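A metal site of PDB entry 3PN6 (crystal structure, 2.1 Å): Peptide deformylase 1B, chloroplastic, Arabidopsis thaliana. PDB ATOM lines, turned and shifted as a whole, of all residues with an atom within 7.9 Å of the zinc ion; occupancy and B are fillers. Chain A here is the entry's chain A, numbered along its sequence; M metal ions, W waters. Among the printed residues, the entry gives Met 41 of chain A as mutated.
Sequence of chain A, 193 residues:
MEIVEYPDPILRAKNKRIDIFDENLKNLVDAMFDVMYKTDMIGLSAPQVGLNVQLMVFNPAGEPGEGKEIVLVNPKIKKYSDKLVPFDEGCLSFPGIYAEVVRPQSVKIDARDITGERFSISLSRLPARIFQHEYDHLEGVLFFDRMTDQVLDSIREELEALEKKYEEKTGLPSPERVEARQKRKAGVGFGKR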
ATOM      1  N   VAL A   4      28.134  -6.026  16.010  1.00  0.00           N
ATOM      2  CA  VAL A   4      28.076  -5.296  17.289  1.00  0.00           C
ATOM      3  C   VAL A   4      26.672  -5.492  17.911  1.00  0.00           C
ATOM      4  O   VAL A   4      25.657  -5.425  17.199  1.00  0.00           O
ATOM      5  CB  VAL A   4      28.402  -3.792  17.057  1.00  0.00           C
ATOM      6  CG1 VAL A   4      28.144  -2.959  18.277  1.00  0.00           C
ATOM      7  CG2 VAL A   4      29.862  -3.630  16.615  1.00  0.00           C
ATOM      8  N   LEU A  11      27.420   1.640  18.805  1.00  0.00           N
ATOM      9  CA  LEU A  11      26.050   1.891  18.325  1.00  0.00           C
ATOM     10  C   LEU A  11      25.480   3.282  18.641  1.00  0.00           C
ATOM     11  O   LEU A  11      24.480   3.654  18.056  1.00  0.00           O
ATOM     12  CB  LEU A  11      25.081   0.787  18.796  1.00  0.00           C
ATOM     13  CG  LEU A  11      25.451  -0.630  18.353  1.00  0.00           C
ATOM     14  CD1 LEU A  11      24.597  -1.691  19.090  1.00  0.00           C
ATOM     15  CD2 LEU A  11      25.375  -0.824  16.767  1.00  0.00           C
ATOM     16  N   MET A  41      19.384 -10.156   5.343  1.00  0.00           N
ATOM     17  CA  MET A  41      18.879  -8.774   5.485  1.00  0.00           C
ATOM     18  C   MET A  41      18.738  -8.075   4.136  1.00  0.00           C
ATOM     19  O   MET A  41      19.306  -8.512   3.142  1.00  0.00           O
ATOM     20  CB  MET A  41      19.812  -7.961   6.384  1.00  0.00           C
ATOM     21  CG  MET A  41      19.720  -8.330   7.865  1.00  0.00           C
ATOM     22  SD  MET A  41      21.075  -7.520   8.694  1.00  0.00           S
ATOM     23  CE  MET A  41      20.423  -5.887   9.133  1.00  0.00           C
ATOM     24  N   GLY A  43      19.196  -4.561   4.138  1.00  0.00           N
ATOM     25  CA  GLY A  43      20.105  -3.414   4.240  1.00  0.00           C
ATOM     26  C   GLY A  43      21.003  -3.544   5.465  1.00  0.00           C
ATOM     27  O   GLY A  43      20.663  -4.286   6.373  1.00  0.00           O
ATOM     28  N   LEU A  44      22.132  -2.831   5.488  1.00  0.00           N
ATOM     29  CA  LEU A  44      23.090  -2.944   6.584  1.00  0.00           C
ATOM     30  C   LEU A  44      23.891  -1.673   6.677  1.00  0.00           C
ATOM     31  O   LEU A  44      24.493  -1.230   5.684  1.00  0.00           O
ATOM     32  CB  LEU A  44      24.042  -4.161   6.395  1.00  0.00           C
ATOM     33  CG  LEU A  44      25.003  -4.424   7.587  1.00  0.00           C
ATOM     34  CD1 LEU A  44      24.249  -4.817   8.866  1.00  0.00           C
ATOM     35  CD2 LEU A  44      26.020  -5.493   7.283  1.00  0.00           C
ATOM     36  N   SER A  45      23.881  -1.069   7.866  1.00  0.00           N
ATOM     37  CA  SER A  45      24.636   0.158   8.122  1.00  0.00           C
ATOM     38  C   SER A  45      25.992  -0.163   8.775  1.00  0.00           C
ATOM     39  O   SER A  45      26.161  -1.227   9.406  1.00  0.00           O
ATOM     40  CB  SER A  45      23.831   1.042   9.056  1.00  0.00           C
ATOM     41  OG  SER A  45      23.744   0.352  10.299  1.00  0.00           O
ATOM     42  N   GLN A  48      26.897  -1.176  12.612  1.00  0.00           N
ATOM     43  CA  GLN A  48      26.486  -2.533  13.009  1.00  0.00           C
ATOM     44  C   GLN A  48      27.575  -3.591  12.802  1.00  0.00           C
ATOM     45  O   GLN A  48      27.560  -4.653  13.451  1.00  0.00           O
ATOM     46  CB  GLN A  48      25.258  -2.960  12.212  1.00  0.00           C
ATOM     47  CG  GLN A  48      24.028  -2.484  12.825  1.00  0.00           C
ATOM     48  CD  GLN A  48      23.017  -3.572  12.883  1.00  0.00           C
ATOM     49  OE1 GLN A  48      22.610  -4.098  11.846  1.00  0.00           O
ATOM     50  NE2 GLN A  48      22.595  -3.931  14.088  1.00  0.00           N
ATOM     51  N   GLU A  89       9.420  -4.850  14.259  1.00  0.00           N
ATOM     52  CA  GLU A  89      10.806  -4.745  13.809  1.00  0.00           C
ATOM     53  C   GLU A  89      11.784  -5.643  14.557  1.00  0.00           C
ATOM     54  O   GLU A  89      11.635  -5.848  15.739  1.00  0.00           O
ATOM     55  CB  GLU A  89      11.289  -3.316  13.953  1.00  0.00           C
ATOM     56  CG  GLU A  89      11.177  -2.546  12.699  1.00  0.00           C
ATOM     57  CD  GLU A  89      11.583  -1.126  12.874  1.00  0.00           C
ATOM     58  OE1 GLU A  89      12.663  -0.857  13.430  1.00  0.00           O
ATOM     59  OE2 GLU A  89      10.773  -0.273  12.482  1.00  0.00           O
ATOM     60  N   GLY A  90      12.794  -6.132  13.844  1.00  0.00           N
ATOM     61  CA  GLY A  90      13.984  -6.735  14.456  1.00  0.00           C
ATOM     62  C   GLY A  90      15.209  -5.842  14.267  1.00  0.00           C
ATOM     63  O   GLY A  90      15.149  -4.798  13.625  1.00  0.00           O
ATOM     64  N   CYS A  91      16.311  -6.265  14.871  1.00  0.00           N
ATOM     65  CA  CYS A  91      17.596  -5.582  14.756  1.00  0.00           C
ATOM     66  C   CYS A  91      18.709  -6.597  15.047  1.00  0.00           C
ATOM     67  O   CYS A  91      18.684  -7.284  16.066  1.00  0.00           O
ATOM     68  CB  CYS A  91      17.677  -4.399  15.738  1.00  0.00           C
ATOM     69  SG  CYS A  91      19.296  -3.542  15.731  1.00  0.00           S
ATOM     70  N   LEU A  92      19.687  -6.671  14.164  1.00  0.00           N
ATOM     71  CA  LEU A  92      20.856  -7.529  14.376  1.00  0.00           C
ATOM     72  C   LEU A  92      21.588  -7.257  15.702  1.00  0.00           C
ATOM     73  O   LEU A  92      22.219  -8.149  16.262  1.00  0.00           O
ATOM     74  CB  LEU A  92      21.858  -7.316  13.259  1.00  0.00           C
ATOM     75  CG  LEU A  92      21.881  -8.247  12.049  1.00  0.00           C
ATOM     76  CD1 LEU A  92      23.158  -7.958  11.295  1.00  0.00           C
ATOM     77  CD2 LEU A  92      21.862  -9.709  12.444  1.00  0.00           C
ATOM     78  N   SER A  93      21.529  -6.015  16.198  1.00  0.00           N
ATOM     79  CA  SER A  93      22.168  -5.683  17.494  1.00  0.00           C
ATOM     80  C   SER A  93      21.434  -6.211  18.742  1.00  0.00           C
ATOM     81  O   SER A  93      21.928  -6.053  19.858  1.00  0.00           O
ATOM     82  CB  SER A  93      22.354  -4.166  17.614  1.00  0.00           C
ATOM     83  OG  SER A  93      23.133  -3.709  16.533  1.00  0.00           O
ATOM     84  N   PHE A  94      20.251  -6.799  18.529  1.00  0.00           N
ATOM     85  CA  PHE A  94      19.380  -7.259  19.623  1.00  0.00           C
ATOM     86  C   PHE A  94      18.879  -8.657  19.216  1.00  0.00           C
ATOM     87  O   PHE A  94      17.732  -8.809  18.796  1.00  0.00           O
ATOM     88  CB  PHE A  94      18.168  -6.308  19.798  1.00  0.00           C
ATOM     89  CG  PHE A  94      18.515  -4.860  20.189  1.00  0.00           C
ATOM     90  CD1 PHE A  94      18.937  -3.937  19.238  1.00  0.00           C
ATOM     91  CD2 PHE A  94      18.333  -4.404  21.490  1.00  0.00           C
ATOM     92  CE1 PHE A  94      19.206  -2.592  19.565  1.00  0.00           C
ATOM     93  CE2 PHE A  94      18.619  -3.064  21.843  1.00  0.00           C
ATOM     94  CZ  PHE A  94      19.060  -2.163  20.863  1.00  0.00           C
ATOM     95  N   ARG A 103       6.408   3.948  11.894  1.00  0.00           N
ATOM     96  CA  ARG A 103       7.292   4.834  11.107  1.00  0.00           C
ATOM     97  C   ARG A 103       6.478   5.253   9.895  1.00  0.00           C
ATOM     98  O   ARG A 103       5.554   4.514   9.533  1.00  0.00           O
ATOM     99  CB  ARG A 103       8.518   4.056  10.585  1.00  0.00           C
ATOM    100  CG  ARG A 103       9.469   3.489  11.629  1.00  0.00           C
ATOM    101  CD  ARG A 103      10.728   2.891  10.931  1.00  0.00           C
ATOM    102  NE  ARG A 103      11.608   2.220  11.899  1.00  0.00           N
ATOM    103  CZ  ARG A 103      12.601   2.815  12.548  1.00  0.00           C
ATOM    104  NH1 ARG A 103      12.873   4.114  12.327  1.00  0.00           N
ATOM    105  NH2 ARG A 103      13.356   2.104  13.398  1.00  0.00           N
ATOM    106  N   ILE A 130      12.970  -1.043   6.296  1.00  0.00           N
ATOM    107  CA  ILE A 130      14.355  -1.446   6.587  1.00  0.00           C
ATOM    108  C   ILE A 130      15.294  -0.268   6.446  1.00  0.00           C
ATOM    109  O   ILE A 130      16.190  -0.105   7.268  1.00  0.00           O
ATOM    110  CB  ILE A 130      14.869  -2.615   5.687  1.00  0.00           C
ATOM    111  CG1 ILE A 130      13.986  -3.866   5.848  1.00  0.00           C
ATOM    112  CG2 ILE A 130      16.336  -2.935   6.030  1.00  0.00           C
ATOM    113  CD1 ILE A 130      13.719  -4.262   7.320  1.00  0.00           C
ATOM    114  N   HIS A 133      15.210   2.069   9.515  1.00  0.00           N
ATOM    115  CA  HIS A 133      15.851   1.402  10.640  1.00  0.00           C
ATOM    116  C   HIS A 133      17.384   1.506  10.557  1.00  0.00           C
ATOM    117  O   HIS A 133      18.065   1.789  11.555  1.00  0.00           O
ATOM    118  CB  HIS A 133      15.448  -0.065  10.689  1.00  0.00           C
ATOM    119  CG  HIS A 133      16.150  -0.831  11.755  1.00  0.00           C
ATOM    120  ND1 HIS A 133      15.564  -1.159  12.955  1.00  0.00           N
ATOM    121  CD2 HIS A 133      17.419  -1.290  11.821  1.00  0.00           C
ATOM    122  CE1 HIS A 133      16.426  -1.811  13.701  1.00  0.00           C
ATOM    123  NE2 HIS A 133      17.572  -1.891  13.042  1.00  0.00           N
ATOM    124  N   GLU A 134      17.937   1.216   9.386  1.00  0.00           N
ATOM    125  CA  GLU A 134      19.404   1.245   9.228  1.00  0.00           C
ATOM    126  C   GLU A 134      19.941   2.676   9.191  1.00  0.00           C
ATOM    127  O   GLU A 134      20.979   2.942   9.748  1.00  0.00           O
ATOM    128  CB  GLU A 134      19.863   0.404   8.016  1.00  0.00           C
ATOM    129  CG  GLU A 134      19.578  -1.124   8.182  1.00  0.00           C
ATOM    130  CD  GLU A 134      20.369  -1.760   9.334  1.00  0.00           C
ATOM    131  OE1 GLU A 134      19.842  -2.676  10.022  1.00  0.00           O
ATOM    132  OE2 GLU A 134      21.525  -1.321   9.578  1.00  0.00           O
ATOM    133  N   ASP A 136      18.618   5.145  10.909  1.00  0.00           N
ATOM    134  CA  ASP A 136      18.661   5.550  12.330  1.00  0.00           C
ATOM    135  C   ASP A 136      20.009   5.158  12.998  1.00  0.00           C
ATOM    136  O   ASP A 136      20.563   5.918  13.784  1.00  0.00           O
ATOM    137  CB  ASP A 136      17.481   4.895  13.088  1.00  0.00           C
ATOM    138  CG  ASP A 136      16.195   5.723  13.039  1.00  0.00           C
ATOM    139  OD1 ASP A 136      16.181   6.835  12.476  1.00  0.00           O
ATOM    140  OD2 ASP A 136      15.177   5.256  13.588  1.00  0.00           O
ATOM    141  N   HIS A 137      20.546   3.967  12.672  1.00  0.00           N
ATOM    142  CA  HIS A 137      21.868   3.520  13.173  1.00  0.00           C
ATOM    143  C   HIS A 137      22.976   4.538  12.832  1.00  0.00           C
ATOM    144  O   HIS A 137      23.914   4.766  13.619  1.00  0.00           O
ATOM    145  CB  HIS A 137      22.256   2.164  12.535  1.00  0.00           C
ATOM    146  CG  HIS A 137      21.682   0.979  13.256  1.00  0.00           C
ATOM    147  ND1 HIS A 137      21.972   0.713  14.574  1.00  0.00           N
ATOM    148  CD2 HIS A 137      20.821   0.007  12.849  1.00  0.00           C
ATOM    149  CE1 HIS A 137      21.318  -0.372  14.953  1.00  0.00           C
ATOM    150  NE2 HIS A 137      20.630  -0.826  13.926  1.00  0.00           N
ATOM    151  N   VAL A 141      20.840   6.255  16.614  1.00  0.00           N
ATOM    152  CA  VAL A 141      19.480   5.950  17.086  1.00  0.00           C
ATOM    153  C   VAL A 141      19.146   4.462  16.947  1.00  0.00           C
ATOM    154  O   VAL A 141      19.390   3.853  15.914  1.00  0.00           O
ATOM    155  CB  VAL A 141      18.393   6.846  16.367  1.00  0.00           C
ATOM    156  CG1 VAL A 141      16.938   6.432  16.758  1.00  0.00           C
ATOM    157  CG2 VAL A 141      18.623   8.291  16.685  1.00  0.00           C
ATOM    158  N   LEU A 142      18.569   3.917  18.015  1.00  0.00           N
ATOM    159  CA  LEU A 142      18.263   2.496  18.158  1.00  0.00           C
ATOM    160  C   LEU A 142      16.730   2.281  18.229  1.00  0.00           C
ATOM    161  O   LEU A 142      15.986   3.155  18.686  1.00  0.00           O
ATOM    162  CB  LEU A 142      19.023   1.893  19.363  1.00  0.00           C
ATOM    163  CG  LEU A 142      20.569   1.898  19.348  1.00  0.00           C
ATOM    164  CD1 LEU A 142      21.154   1.145  20.551  1.00  0.00           C
ATOM    165  CD2 LEU A 142      21.195   1.349  18.033  1.00  0.00           C
ATOM    166  N   PHE A 143      16.263   1.139  17.718  1.00  0.00           N
ATOM    167  CA  PHE A 143      14.796   0.963  17.483  1.00  0.00           C
ATOM    168  C   PHE A 143      13.876   1.065  18.699  1.00  0.00           C
ATOM    169  O   PHE A 143      12.728   1.434  18.559  1.00  0.00           O
ATOM    170  CB  PHE A 143      14.458  -0.247  16.576  1.00  0.00           C
ATOM    171  CG  PHE A 143      14.553  -1.637  17.251  1.00  0.00           C
ATOM    172  CD1 PHE A 143      13.727  -2.666  16.818  1.00  0.00           C
ATOM    173  CD2 PHE A 143      15.502  -1.924  18.235  1.00  0.00           C
ATOM    174  CE1 PHE A 143      13.798  -3.941  17.378  1.00  0.00           C
ATOM    175  CE2 PHE A 143      15.575  -3.201  18.804  1.00  0.00           C
ATOM    176  CZ  PHE A 143      14.728  -4.214  18.358  1.00  0.00           C
HETATM  177 ZN    ZN M   1      19.390  -2.499  13.788  1.00  0.00          ZN
HETATM  178  O   HOH W   1      20.011  -3.477  12.340  1.00  0.00           O
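Water W1 lies within hydrogen-bond range of the side-chain carboxylate (OE1) of Glu 134 and the side-chain amide oxygen (OE1) of Gln 48.
The side-chain carboxylate (OE1) of Glu 89 is in hydrogen-bond range of a ring nitrogen (ND1) of His 133 (3.0 Å).
The backbone carbonyl oxygen (O) of Gln 48 lies within hydrogen-bond range of the backbone NH (N) of Val 4 (3.0 Å).
The side-chain sulfur of Cys 91 lies close to the backbone NH of Ser 93 (3.4 Å).
The side-chain amide nitrogen (NE2) of Gln 48 is in hydrogen-bond range of the side-chain hydroxyl (OG) of Ser 93.
The side-chain carboxylate of Glu 134 lies within hydrogen-bond range of the side-chain hydroxyl of Ser 45.
SG of Cys 91 sits close to NE2 of Gln 48, at 3.7 Å.
Gln 48 touches the zinc ion.
OE1 of Glu 134 touches the zinc ion (3.8 Å).
The nearest printed residue that does not touch the zinc ion is Leu 92 (4.2 Å).
The zinc ion is bound by water W1, at 1.9 Å.
The zinc ion is bound by a ring nitrogen (NE2) of His 133 (2.1 Å).
NE2 of His 137 binds the zinc ion, at 2.1 Å.
SG of Cys 91 is bound to the zinc ion (2.2 Å).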
